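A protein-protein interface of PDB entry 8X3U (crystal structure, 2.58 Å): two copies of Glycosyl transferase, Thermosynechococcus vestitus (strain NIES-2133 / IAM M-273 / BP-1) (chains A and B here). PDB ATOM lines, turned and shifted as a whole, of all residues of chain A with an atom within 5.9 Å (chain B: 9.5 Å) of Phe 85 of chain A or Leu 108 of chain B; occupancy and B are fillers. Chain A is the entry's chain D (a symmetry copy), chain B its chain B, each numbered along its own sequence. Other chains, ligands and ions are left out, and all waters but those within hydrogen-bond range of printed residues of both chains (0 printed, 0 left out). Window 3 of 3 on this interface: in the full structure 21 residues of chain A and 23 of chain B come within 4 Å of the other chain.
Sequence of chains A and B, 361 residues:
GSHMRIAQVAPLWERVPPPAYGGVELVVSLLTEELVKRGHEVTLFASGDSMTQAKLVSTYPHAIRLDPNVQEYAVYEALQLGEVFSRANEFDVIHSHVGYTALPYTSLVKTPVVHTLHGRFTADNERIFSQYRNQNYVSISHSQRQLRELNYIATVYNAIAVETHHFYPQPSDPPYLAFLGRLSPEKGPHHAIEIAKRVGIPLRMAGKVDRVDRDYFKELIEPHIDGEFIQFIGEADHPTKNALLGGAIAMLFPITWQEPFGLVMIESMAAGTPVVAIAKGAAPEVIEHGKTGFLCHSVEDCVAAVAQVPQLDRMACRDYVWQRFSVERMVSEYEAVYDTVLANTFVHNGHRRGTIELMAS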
ATOM      1  N   GLN A  80      13.629 -24.239  -3.136  1.00  0.00           N
ATOM      2  CA  GLN A  80      12.228 -23.889  -3.351  1.00  0.00           C
ATOM      3  C   GLN A  80      12.046 -23.042  -4.604  1.00  0.00           C
ATOM      4  O   GLN A  80      11.149 -23.300  -5.415  1.00  0.00           O
ATOM      5  CB  GLN A  80      11.692 -23.157  -2.125  1.00  0.00           C
ATOM      6  CG  GLN A  80      10.312 -22.576  -2.300  1.00  0.00           C
ATOM      7  CD  GLN A  80       9.635 -22.342  -0.973  1.00  0.00           C
ATOM      8  OE1 GLN A  80       9.010 -23.245  -0.416  1.00  0.00           O
ATOM      9  NE2 GLN A  80       9.767 -21.131  -0.448  1.00  0.00           N
ATOM     10  N   LEU A  81      12.879 -22.011  -4.772  1.00  0.00           N
ATOM     11  CA  LEU A  81      12.758 -21.154  -5.947  1.00  0.00           C
ATOM     12  C   LEU A  81      13.012 -21.929  -7.233  1.00  0.00           C
ATOM     13  O   LEU A  81      12.387 -21.648  -8.262  1.00  0.00           O
ATOM     14  CB  LEU A  81      13.711 -19.965  -5.825  1.00  0.00           C
ATOM     15  CG  LEU A  81      13.293 -18.958  -4.750  1.00  0.00           C
ATOM     16  CD1 LEU A  81      14.265 -17.787  -4.669  1.00  0.00           C
ATOM     17  CD2 LEU A  81      11.871 -18.471  -5.000  1.00  0.00           C
ATOM     18  N   GLY A  82      13.919 -22.906  -7.194  1.00  0.00           N
ATOM     19  CA  GLY A  82      14.105 -23.777  -8.341  1.00  0.00           C
ATOM     20  C   GLY A  82      12.864 -24.589  -8.657  1.00  0.00           C
ATOM     21  O   GLY A  82      12.497 -24.750  -9.824  1.00  0.00           O
ATOM     22  N   GLU A  83      12.212 -25.122  -7.620  1.00  0.00           N
ATOM     23  CA  GLU A  83      10.998 -25.909  -7.817  1.00  0.00           C
ATOM     24  C   GLU A  83       9.893 -25.087  -8.471  1.00  0.00           C
ATOM     25  O   GLU A  83       9.223 -25.555  -9.398  1.00  0.00           O
ATOM     26  CB  GLU A  83      10.517 -26.462  -6.473  1.00  0.00           C
ATOM     27  CG  GLU A  83      11.138 -27.790  -6.079  1.00  0.00           C
ATOM     28  CD  GLU A  83      11.039 -28.826  -7.178  1.00  0.00           C
ATOM     29  OE1 GLU A  83       9.947 -28.967  -7.768  1.00  0.00           O
ATOM     30  OE2 GLU A  83      12.055 -29.498  -7.453  1.00  0.00           O
ATOM     31  N   VAL A  84       9.691 -23.854  -8.005  1.00  0.00           N
ATOM     32  CA  VAL A  84       8.576 -23.041  -8.491  1.00  0.00           C
ATOM     33  C   VAL A  84       8.732 -22.749  -9.977  1.00  0.00           C
ATOM     34  O   VAL A  84       7.872 -23.097 -10.796  1.00  0.00           O
ATOM     35  CB  VAL A  84       8.459 -21.742  -7.675  1.00  0.00           C
ATOM     36  CG1 VAL A  84       7.332 -20.873  -8.219  1.00  0.00           C
ATOM     37  CG2 VAL A  84       8.243 -22.058  -6.200  1.00  0.00           C
ATOM     38  N   PHE A  85       9.841 -22.106 -10.349  1.00  0.00           N
ATOM     39  CA  PHE A  85      10.014 -21.606 -11.705  1.00  0.00           C
ATOM     40  C   PHE A  85      10.340 -22.704 -12.710  1.00  0.00           C
ATOM     41  O   PHE A  85      10.186 -22.482 -13.917  1.00  0.00           O
ATOM     42  CB  PHE A  85      11.098 -20.527 -11.719  1.00  0.00           C
ATOM     43  CG  PHE A  85      10.758 -19.334 -10.876  1.00  0.00           C
ATOM     44  CD1 PHE A  85       9.839 -18.397 -11.317  1.00  0.00           C
ATOM     45  CD2 PHE A  85      11.330 -19.167  -9.627  1.00  0.00           C
ATOM     46  CE1 PHE A  85       9.515 -17.303 -10.534  1.00  0.00           C
ATOM     47  CE2 PHE A  85      11.007 -18.080  -8.840  1.00  0.00           C
ATOM     48  CZ  PHE A  85      10.102 -17.144  -9.294  1.00  0.00           C
ATOM     49  N   SER A  86      10.788 -23.875 -12.254  1.00  0.00           N
ATOM     50  CA  SER A  86      10.847 -25.018 -13.156  1.00  0.00           C
ATOM     51  C   SER A  86       9.458 -25.492 -13.558  1.00  0.00           C
ATOM     52  O   SER A  86       9.312 -26.133 -14.605  1.00  0.00           O
ATOM     53  CB  SER A  86      11.622 -26.171 -12.514  1.00  0.00           C
ATOM     54  OG  SER A  86      10.903 -26.735 -11.428  1.00  0.00           O
ATOM     55  N   ARG A  87       8.441 -25.200 -12.744  1.00  0.00           N
ATOM     56  CA  ARG A  87       7.059 -25.566 -13.024  1.00  0.00           C
ATOM     57  C   ARG A  87       6.192 -24.351 -13.335  1.00  0.00           C
ATOM     58  O   ARG A  87       4.970 -24.411 -13.163  1.00  0.00           O
ATOM     59  CB  ARG A  87       6.471 -26.340 -11.847  1.00  0.00           C
ATOM     60  CG  ARG A  87       7.166 -27.664 -11.560  1.00  0.00           C
ATOM     61  CD  ARG A  87       7.257 -27.925 -10.063  1.00  0.00           C
ATOM     62  NE  ARG A  87       5.998 -28.403  -9.502  1.00  0.00           N
ATOM     63  CZ  ARG A  87       5.894 -29.047  -8.344  1.00  0.00           C
ATOM     64  NH1 ARG A  87       6.976 -29.287  -7.616  1.00  0.00           N
ATOM     65  NH2 ARG A  87       4.706 -29.448  -7.910  1.00  0.00           N
ATOM     66  N   ALA A  88       6.805 -23.248 -13.786  1.00  0.00           N
ATOM     67  CA  ALA A  88       6.091 -21.980 -13.934  1.00  0.00           C
ATOM     68  C   ALA A  88       4.843 -22.111 -14.805  1.00  0.00           C
ATOM     69  O   ALA A  88       3.791 -21.535 -14.491  1.00  0.00           O
ATOM     70  CB  ALA A  88       7.032 -20.917 -14.504  1.00  0.00           C
ATOM     71  N   ASN A  89       4.939 -22.854 -15.907  1.00  0.00           N
ATOM     72  CA  ASN A  89       3.831 -22.961 -16.846  1.00  0.00           C
ATOM     73  C   ASN A  89       2.751 -23.927 -16.354  1.00  0.00           C
ATOM     74  O   ASN A  89       1.816 -24.241 -17.096  1.00  0.00           O
ATOM     75  CB  ASN A  89       4.360 -23.373 -18.223  1.00  0.00           C
ATOM     76  CG  ASN A  89       3.444 -22.944 -19.377  1.00  0.00           C
ATOM     77  OD1 ASN A  89       2.223 -23.074 -19.319  1.00  0.00           O
ATOM     78  ND2 ASN A  89       4.051 -22.399 -20.429  1.00  0.00           N
ATOM     79  N   ILE A  94       2.260 -16.552 -10.202  1.00  0.00           N
ATOM     80  CA  ILE A  94       3.104 -16.920  -9.073  1.00  0.00           C
ATOM     81  C   ILE A  94       3.111 -15.758  -8.092  1.00  0.00           C
ATOM     82  O   ILE A  94       3.452 -14.628  -8.463  1.00  0.00           O
ATOM     83  CB  ILE A  94       4.534 -17.267  -9.522  1.00  0.00           C
ATOM     84  CG1 ILE A  94       4.539 -18.555 -10.347  1.00  0.00           C
ATOM     85  CG2 ILE A  94       5.453 -17.388  -8.317  1.00  0.00           C
ATOM     86  CD1 ILE A  94       5.650 -18.620 -11.365  1.00  0.00           C
ATOM     87  N   ALA A 102      13.710 -13.537  -5.666  1.00  0.00           N
ATOM     88  CA  ALA A 102      12.934 -14.081  -6.771  1.00  0.00           C
ATOM     89  C   ALA A 102      12.902 -13.175  -7.994  1.00  0.00           C
ATOM     90  O   ALA A 102      12.397 -13.595  -9.041  1.00  0.00           O
ATOM     91  CB  ALA A 102      11.497 -14.362  -6.314  1.00  0.00           C
ATOM     92  N   TYR A 105      14.562 -14.403 -11.235  1.00  0.00           N
ATOM     93  CA  TYR A 105      13.821 -15.510 -11.825  1.00  0.00           C
ATOM     94  C   TYR A 105      12.664 -15.014 -12.681  1.00  0.00           C
ATOM     95  O   TYR A 105      12.295 -15.671 -13.662  1.00  0.00           O
ATOM     96  CB  TYR A 105      13.288 -16.434 -10.733  1.00  0.00           C
ATOM     97  CG  TYR A 105      14.345 -17.234 -10.016  1.00  0.00           C
ATOM     98  CD1 TYR A 105      14.914 -18.355 -10.604  1.00  0.00           C
ATOM     99  CD2 TYR A 105      14.774 -16.871  -8.746  1.00  0.00           C
ATOM    100  CE1 TYR A 105      15.883 -19.090  -9.948  1.00  0.00           C
ATOM    101  CE2 TYR A 105      15.741 -17.600  -8.082  1.00  0.00           C
ATOM    102  CZ  TYR A 105      16.292 -18.708  -8.689  1.00  0.00           C
ATOM    103  OH  TYR A 105      17.257 -19.439  -8.034  1.00  0.00           O
ATOM    104  N   THR A 106      12.085 -13.863 -12.329  1.00  0.00           N
ATOM    105  CA  THR A 106      10.883 -13.395 -13.012  1.00  0.00           C
ATOM    106  C   THR A 106      11.176 -13.036 -14.462  1.00  0.00           C
ATOM    107  O   THR A 106      10.344 -13.272 -15.346  1.00  0.00           O
ATOM    108  CB  THR A 106      10.298 -12.192 -12.273  1.00  0.00           C
ATOM    109  OG1 THR A 106      10.216 -12.484 -10.872  1.00  0.00           O
ATOM    110  CG2 THR A 106       8.915 -11.850 -12.811  1.00  0.00           C
ATOM    111  N   LEU A 108      13.164 -14.536 -16.321  1.00  0.00           N
ATOM    112  CA  LEU A 108      13.556 -15.754 -17.014  1.00  0.00           C
ATOM    113  C   LEU A 108      12.394 -16.699 -17.269  1.00  0.00           C
ATOM    114  O   LEU A 108      12.561 -17.675 -18.010  1.00  0.00           O
ATOM    115  CB  LEU A 108      14.632 -16.496 -16.213  1.00  0.00           C
ATOM    116  CG  LEU A 108      16.056 -15.953 -16.321  1.00  0.00           C
ATOM    117  CD1 LEU A 108      16.934 -16.561 -15.241  1.00  0.00           C
ATOM    118  CD2 LEU A 108      16.625 -16.222 -17.705  1.00  0.00           C
ATOM    119  N   VAL A 109      11.228 -16.436 -16.686  1.00  0.00           N
ATOM    120  CA  VAL A 109      10.071 -17.301 -16.857  1.00  0.00           C
ATOM    121  C   VAL A 109       8.977 -16.535 -17.582  1.00  0.00           C
ATOM    122  O   VAL A 109       8.990 -15.306 -17.682  1.00  0.00           O
ATOM    123  CB  VAL A 109       9.543 -17.869 -15.526  1.00  0.00           C
ATOM    124  CG1 VAL A 109      10.576 -18.785 -14.905  1.00  0.00           C
ATOM    125  CG2 VAL A 109       9.153 -16.747 -14.582  1.00  0.00           C
ATOM    126  N   LYS A 110       8.025 -17.298 -18.109  1.00  0.00           N
ATOM    127  CA  LYS A 110       6.962 -16.728 -18.921  1.00  0.00           C
ATOM    128  C   LYS A 110       5.720 -16.401 -18.111  1.00  0.00           C
ATOM    129  O   LYS A 110       5.020 -15.435 -18.427  1.00  0.00           O
ATOM    130  CB  LYS A 110       6.619 -17.701 -20.056  1.00  0.00           C
ATOM    131  CG  LYS A 110       7.678 -17.691 -21.170  1.00  0.00           C
ATOM    132  CD  LYS A 110       8.957 -18.396 -20.684  1.00  0.00           C
ATOM    133  CE  LYS A 110      10.103 -18.433 -21.680  1.00  0.00           C
ATOM    134  NZ  LYS A 110      11.303 -19.008 -21.005  1.00  0.00           N
ATOM    135  N   VAL A 113       4.740 -12.873 -12.461  1.00  0.00           N
ATOM    136  CA  VAL A 113       4.957 -13.035 -11.028  1.00  0.00           C
ATOM    137  C   VAL A 113       4.547 -11.760 -10.307  1.00  0.00           C
ATOM    138  O   VAL A 113       4.807 -10.651 -10.786  1.00  0.00           O
ATOM    139  CB  VAL A 113       6.430 -13.380 -10.717  1.00  0.00           C
ATOM    140  CG1 VAL A 113       6.653 -13.513  -9.215  1.00  0.00           C
ATOM    141  CG2 VAL A 113       6.846 -14.652 -11.438  1.00  0.00           C
ATOM    142  N   PHE B  85      22.506 -14.777 -16.590  1.00  0.00           N
ATOM    143  CA  PHE B  85      21.609 -15.682 -17.294  1.00  0.00           C
ATOM    144  C   PHE B  85      20.596 -14.957 -18.172  1.00  0.00           C
ATOM    145  O   PHE B  85      20.016 -15.580 -19.067  1.00  0.00           O
ATOM    146  CB  PHE B  85      20.903 -16.590 -16.286  1.00  0.00           C
ATOM    147  CG  PHE B  85      21.826 -17.576 -15.629  1.00  0.00           C
ATOM    148  CD1 PHE B  85      22.555 -17.222 -14.505  1.00  0.00           C
ATOM    149  CD2 PHE B  85      21.985 -18.849 -16.152  1.00  0.00           C
ATOM    150  CE1 PHE B  85      23.411 -18.125 -13.906  1.00  0.00           C
ATOM    151  CE2 PHE B  85      22.837 -19.756 -15.560  1.00  0.00           C
ATOM    152  CZ  PHE B  85      23.553 -19.394 -14.435  1.00  0.00           C
ATOM    153  N   SER B  86      20.367 -13.664 -17.942  1.00  0.00           N
ATOM    154  CA  SER B  86      19.626 -12.873 -18.916  1.00  0.00           C
ATOM    155  C   SER B  86      20.399 -12.693 -20.216  1.00  0.00           C
ATOM    156  O   SER B  86      19.792 -12.384 -21.247  1.00  0.00           O
ATOM    157  CB  SER B  86      19.268 -11.507 -18.326  1.00  0.00           C
ATOM    158  OG  SER B  86      20.361 -10.960 -17.608  1.00  0.00           O
ATOM    159  N   ALA B  88      22.425 -15.159 -21.495  1.00  0.00           N
ATOM    160  CA  ALA B  88      22.930 -16.514 -21.710  1.00  0.00           C
ATOM    161  C   ALA B  88      23.379 -16.747 -23.148  1.00  0.00           C
ATOM    162  O   ALA B  88      24.412 -17.373 -23.395  1.00  0.00           O
ATOM    163  CB  ALA B  88      21.850 -17.531 -21.326  1.00  0.00           C
ATOM    164  N   ASN B  89      22.584 -16.304 -24.111  1.00  0.00           N
ATOM    165  CA  ASN B  89      22.854 -16.497 -25.535  1.00  0.00           C
ATOM    166  C   ASN B  89      23.867 -15.530 -26.096  1.00  0.00           C
ATOM    167  O   ASN B  89      24.092 -15.531 -27.312  1.00  0.00           O
ATOM    168  CB  ASN B  89      21.538 -16.478 -26.321  1.00  0.00           C
ATOM    169  CG  ASN B  89      20.921 -17.849 -26.410  1.00  0.00           C
ATOM    170  OD1 ASN B  89      21.602 -18.801 -26.814  1.00  0.00           O
ATOM    171  ND2 ASN B  89      19.691 -18.004 -25.914  1.00  0.00           N
ATOM    172  N   ILE B  94      28.980 -20.887 -19.712  1.00  0.00           N
ATOM    173  CA  ILE B  94      29.059 -20.088 -18.495  1.00  0.00           C
ATOM    174  C   ILE B  94      29.852 -20.872 -17.462  1.00  0.00           C
ATOM    175  O   ILE B  94      29.519 -22.025 -17.161  1.00  0.00           O
ATOM    176  CB  ILE B  94      27.661 -19.730 -17.959  1.00  0.00           C
ATOM    177  CG1 ILE B  94      26.852 -18.988 -19.025  1.00  0.00           C
ATOM    178  CG2 ILE B  94      27.772 -18.898 -16.691  1.00  0.00           C
ATOM    179  CD1 ILE B  94      25.423 -18.712 -18.620  1.00  0.00           C
ATOM    180  N   ALA B 102      23.822 -20.969  -8.209  1.00  0.00           N
ATOM    181  CA  ALA B 102      23.635 -20.903  -9.649  1.00  0.00           C
ATOM    182  C   ALA B 102      22.864 -22.085 -10.205  1.00  0.00           C
ATOM    183  O   ALA B 102      22.629 -22.123 -11.416  1.00  0.00           O
ATOM    184  CB  ALA B 102      24.983 -20.823 -10.366  1.00  0.00           C
ATOM    185  N   LEU B 103      22.540 -23.085  -9.378  1.00  0.00           N
ATOM    186  CA  LEU B 103      21.915 -24.303  -9.895  1.00  0.00           C
ATOM    187  C   LEU B 103      20.476 -24.132 -10.389  1.00  0.00           C
ATOM    188  O   LEU B 103      20.179 -24.596 -11.504  1.00  0.00           O
ATOM    189  CB  LEU B 103      22.036 -25.413  -8.846  1.00  0.00           C
ATOM    190  CG  LEU B 103      23.385 -25.726  -8.186  1.00  0.00           C
ATOM    191  CD1 LEU B 103      23.321 -27.057  -7.447  1.00  0.00           C
ATOM    192  CD2 LEU B 103      24.519 -25.743  -9.195  1.00  0.00           C
ATOM    193  N   PRO B 104      19.533 -23.562  -9.628  1.00  0.00           N
ATOM    194  CA  PRO B 104      18.199 -23.326 -10.215  1.00  0.00           C
ATOM    195  C   PRO B 104      18.188 -22.391 -11.426  1.00  0.00           C
ATOM    196  O   PRO B 104      17.260 -22.482 -12.237  1.00  0.00           O
ATOM    197  CB  PRO B 104      17.366 -22.801  -9.032  1.00  0.00           C
ATOM    198  CG  PRO B 104      18.280 -22.752  -7.839  1.00  0.00           C
ATOM    199  CD  PRO B 104      19.463 -23.616  -8.154  1.00  0.00           C
ATOM    200  N   TYR B 105      19.191 -21.533 -11.615  1.00  0.00           N
ATOM    201  CA  TYR B 105      19.224 -20.751 -12.850  1.00  0.00           C
ATOM    202  C   TYR B 105      19.617 -21.612 -14.050  1.00  0.00           C
ATOM    203  O   TYR B 105      19.173 -21.350 -15.177  1.00  0.00           O
ATOM    204  CB  TYR B 105      20.188 -19.575 -12.707  1.00  0.00           C
ATOM    205  CG  TYR B 105      19.761 -18.554 -11.681  1.00  0.00           C
ATOM    206  CD1 TYR B 105      20.131 -18.687 -10.348  1.00  0.00           C
ATOM    207  CD2 TYR B 105      18.988 -17.458 -12.042  1.00  0.00           C
ATOM    208  CE1 TYR B 105      19.746 -17.754  -9.402  1.00  0.00           C
ATOM    209  CE2 TYR B 105      18.596 -16.521 -11.104  1.00  0.00           C
ATOM    210  CZ  TYR B 105      18.980 -16.673  -9.786  1.00  0.00           C
ATOM    211  OH  TYR B 105      18.596 -15.745  -8.845  1.00  0.00           O
ATOM    212  N   THR B 106      20.429 -22.650 -13.828  1.00  0.00           N
ATOM    213  CA  THR B 106      20.981 -23.434 -14.931  1.00  0.00           C
ATOM    214  C   THR B 106      19.895 -24.215 -15.666  1.00  0.00           C
ATOM    215  O   THR B 106      19.950 -24.360 -16.895  1.00  0.00           O
ATOM    216  CB  THR B 106      22.063 -24.371 -14.390  1.00  0.00           C
ATOM    217  OG1 THR B 106      23.113 -23.590 -13.807  1.00  0.00           O
ATOM    218  CG2 THR B 106      22.645 -25.233 -15.492  1.00  0.00           C
ATOM    219  N   SER B 107      18.893 -24.714 -14.940  1.00  0.00           N
ATOM    220  CA  SER B 107      17.797 -25.439 -15.570  1.00  0.00           C
ATOM    221  C   SER B 107      16.886 -24.539 -16.401  1.00  0.00           C
ATOM    222  O   SER B 107      16.033 -25.058 -17.128  1.00  0.00           O
ATOM    223  CB  SER B 107      16.966 -26.167 -14.508  1.00  0.00           C
ATOM    224  OG  SER B 107      15.963 -25.321 -13.968  1.00  0.00           O
ATOM    225  N   LEU B 108      17.038 -23.217 -16.310  1.00  0.00           N
ATOM    226  CA  LEU B 108      16.134 -22.280 -16.968  1.00  0.00           C
ATOM    227  C   LEU B 108      16.717 -21.649 -18.226  1.00  0.00           C
ATOM    228  O   LEU B 108      15.984 -20.976 -18.961  1.00  0.00           O
ATOM    229  CB  LEU B 108      15.718 -21.177 -15.983  1.00  0.00           C
ATOM    230  CG  LEU B 108      14.795 -21.600 -14.829  1.00  0.00           C
ATOM    231  CD1 LEU B 108      14.183 -20.383 -14.150  1.00  0.00           C
ATOM    232  CD2 LEU B 108      13.702 -22.557 -15.298  1.00  0.00           C
ATOM    233  N   VAL B 109      18.009 -21.839 -18.479  1.00  0.00           N
ATOM    234  CA  VAL B 109      18.672 -21.322 -19.663  1.00  0.00           C
ATOM    235  C   VAL B 109      19.189 -22.514 -20.454  1.00  0.00           C
ATOM    236  O   VAL B 109      19.312 -23.631 -19.943  1.00  0.00           O
ATOM    237  CB  VAL B 109      19.816 -20.342 -19.321  1.00  0.00           C
ATOM    238  CG1 VAL B 109      19.299 -19.181 -18.472  1.00  0.00           C
ATOM    239  CG2 VAL B 109      20.923 -21.075 -18.610  1.00  0.00           C
ATOM    240  N   LYS B 110      19.468 -22.259 -21.727  1.00  0.00           N
ATOM    241  CA  LYS B 110      19.938 -23.258 -22.678  1.00  0.00           C
ATOM    242  C   LYS B 110      21.455 -23.305 -22.796  1.00  0.00           C
ATOM    243  O   LYS B 110      22.025 -24.387 -22.988  1.00  0.00           O
ATOM    244  CB  LYS B 110      19.258 -22.980 -24.020  1.00  0.00           C
ATOM    245  CG  LYS B 110      17.773 -23.308 -23.869  1.00  0.00           C
ATOM    246  CD  LYS B 110      16.930 -22.952 -25.022  1.00  0.00           C
ATOM    247  CE  LYS B 110      15.509 -23.393 -24.798  1.00  0.00           C
ATOM    248  NZ  LYS B 110      14.637 -22.974 -25.924  1.00  0.00           N
ATOM    249  N   THR B 111      22.111 -22.173 -22.573  1.00  0.00           N
ATOM    250  CA  THR B 111      23.560 -22.125 -22.579  1.00  0.00           C
ATOM    251  C   THR B 111      24.112 -23.045 -21.499  1.00  0.00           C
ATOM    252  O   THR B 111      23.721 -22.929 -20.326  1.00  0.00           O
ATOM    253  CB  THR B 111      24.038 -20.694 -22.351  1.00  0.00           C
ATOM    254  OG1 THR B 111      23.515 -19.850 -23.384  1.00  0.00           O
ATOM    255  CG2 THR B 111      25.551 -20.642 -22.390  1.00  0.00           C
ATOM    256  N   PRO B 112      25.006 -23.967 -21.844  1.00  0.00           N
ATOM    257  CA  PRO B 112      25.545 -24.882 -20.836  1.00  0.00           C
ATOM    258  C   PRO B 112      26.392 -24.141 -19.818  1.00  0.00           C
ATOM    259  O   PRO B 112      27.118 -23.199 -20.148  1.00  0.00           O
ATOM    260  CB  PRO B 112      26.385 -25.865 -21.661  1.00  0.00           C
ATOM    261  CG  PRO B 112      26.687 -25.140 -22.929  1.00  0.00           C
ATOM    262  CD  PRO B 112      25.500 -24.270 -23.196  1.00  0.00           C
ATOM    263  N   VAL B 113      26.289 -24.580 -18.568  1.00  0.00           N
ATOM    264  CA  VAL B 113      26.965 -23.952 -17.444  1.00  0.00           C
ATOM    265  C   VAL B 113      27.930 -24.958 -16.838  1.00  0.00           C
ATOM    266  O   VAL B 113      27.602 -26.140 -16.695  1.00  0.00           O
ATOM    267  CB  VAL B 113      25.953 -23.462 -16.386  1.00  0.00           C
ATOM    268  CG1 VAL B 113      26.657 -22.686 -15.284  1.00  0.00           C
ATOM    269  CG2 VAL B 113      24.868 -22.619 -17.036  1.00  0.00           C
ATOM    270  N   TYR B 132      20.385 -31.443  -8.341  1.00  0.00           N
ATOM    271  CA  TYR B 132      20.906 -30.958  -9.612  1.00  0.00           C
ATOM    272  C   TYR B 132      22.152 -31.739 -10.008  1.00  0.00           C
ATOM    273  O   TYR B 132      23.102 -31.194 -10.576  1.00  0.00           O
ATOM    274  CB  TYR B 132      21.196 -29.461  -9.538  1.00  0.00           C
ATOM    275  CG  TYR B 132      19.953 -28.606  -9.442  1.00  0.00           C
ATOM    276  CD1 TYR B 132      19.284 -28.187 -10.584  1.00  0.00           C
ATOM    277  CD2 TYR B 132      19.442 -28.225  -8.208  1.00  0.00           C
ATOM    278  CE1 TYR B 132      18.146 -27.406 -10.500  1.00  0.00           C
ATOM    279  CE2 TYR B 132      18.305 -27.445  -8.115  1.00  0.00           C
ATOM    280  CZ  TYR B 132      17.662 -27.039  -9.264  1.00  0.00           C
ATOM    281  OH  TYR B 132      16.529 -26.263  -9.178  1.00  0.00           O
ATOM    282  N   GLN B 135      24.288 -31.952 -13.610  1.00  0.00           N
ATOM    283  CA  GLN B 135      24.932 -30.776 -14.172  1.00  0.00           C
ATOM    284  C   GLN B 135      26.446 -30.969 -14.198  1.00  0.00           C
ATOM    285  O   GLN B 135      26.993 -31.907 -13.612  1.00  0.00           O
ATOM    286  CB  GLN B 135      24.540 -29.522 -13.386  1.00  0.00           C
ATOM    287  CG  GLN B 135      23.107 -29.083 -13.658  1.00  0.00           C
ATOM    288  CD  GLN B 135      22.747 -27.778 -12.979  1.00  0.00           C
ATOM    289  OE1 GLN B 135      23.616 -27.049 -12.504  1.00  0.00           O
ATOM    290  NE2 GLN B 135      21.455 -27.476 -12.933  1.00  0.00           N
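The backbone carbonyl oxygen (O) of Gly 82 of chain A lies within hydrogen-bond range of the side-chain hydroxyl (OG) of Ser 86 of chain A (3.0 Å).
Among the printed residues, merely in contact across the chains: Gly 82 of chain A with Pro 104 of chain B (3.5 Å), Gly 82 of chain A with Tyr 132 of chain B (3.6 Å), Phe 85 of chain A with Leu 108 of chain B (3.8 Å), Tyr 105 of chain A with Pro 104 of chain B (3.5 Å), Tyr 105 of chain A with Tyr 105 of chain B (3.3 Å), Leu 108 of chain A with Phe 85 of chain B (3.7 Å) and Leu 108 of chain A with Tyr 105 of chain B (3.9 Å).
Of the printed residues of chain A, Leu 108 of chain B touches Phe 85 (3.8 Å).
Printed residues of chain B within 4 Å of Gly 82 of chain A: Pro 104 (3.5 Å) and Tyr 132 (3.6 Å).
No residue of chain B comes within 4 Å of Val 84 of chain A.
Printed residues of chain B within 4 Å of Leu 108 of chain A: Phe 85 (3.7 Å) and Tyr 105 (3.9 Å).
Printed residues of chain B within 4 Å of Tyr 105 of chain A: Pro 104 (3.5 Å) and Tyr 105 (3.3 Å).
Of the printed residues of chain A, Phe 85 of chain B touches Leu 108 (3.7 Å).
Of the printed residues of chain A, Pro 104 of chain B touches Gly 82 (3.5 Å) and Tyr 105 (3.5 Å).
Thr 111 of chain B touches none of the printed residues of chain A.
Asn 89 of chain B touches none of the printed residues of chain A.
The nearest printed residue of chain A that does not touch Leu 108 of chain B is Val 109 of chain A (4.02 Å).
The nearest printed residue of chain A that does not touch Tyr 105 of chain B is Ala 102 of chain A (6.2 Å).
Of the 19 printed residues of chain B, 5 touch a printed residue of chain A.
Printed residues of chain B that touch a printed residue of chain A: Phe 85, Pro 104, Tyr 105, Leu 108 and Tyr 132.
Along chain B the printed residues that touch a printed residue of chain A span positions 85 to 132.
Hydrophobic or aromatic side chains of chain A within 4 Å of the printed part of chain B: Phe 85, Tyr 105 and Leu 108.
Among the printed residues, no Asp or Glu carboxylate lies within 4 Å of a Lys or Arg side-chain nitrogen of the other chain.
Phe 85 of chain A touches Leu 108 of chain B, and with the chains exchanged Leu 108 of chain A touches Phe 85 of chain B.
Tyr 105 of chain A touches its own counterpart, Tyr 105 of chain B.
Leu 108 of chain A touches Tyr 105 of chain B, but with the chains exchanged Tyr 105 of chain A does not touch Leu 108 of chain B (4.1 Å).
Positions printed for both chains: 85, 86, 88, 89, 94, 102, 105, 106, 108, 109, 110 and 113.
Of the 7 pairs that touch across the chains among the printed residues, 3 have their exchanged pair printed and touching as well.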
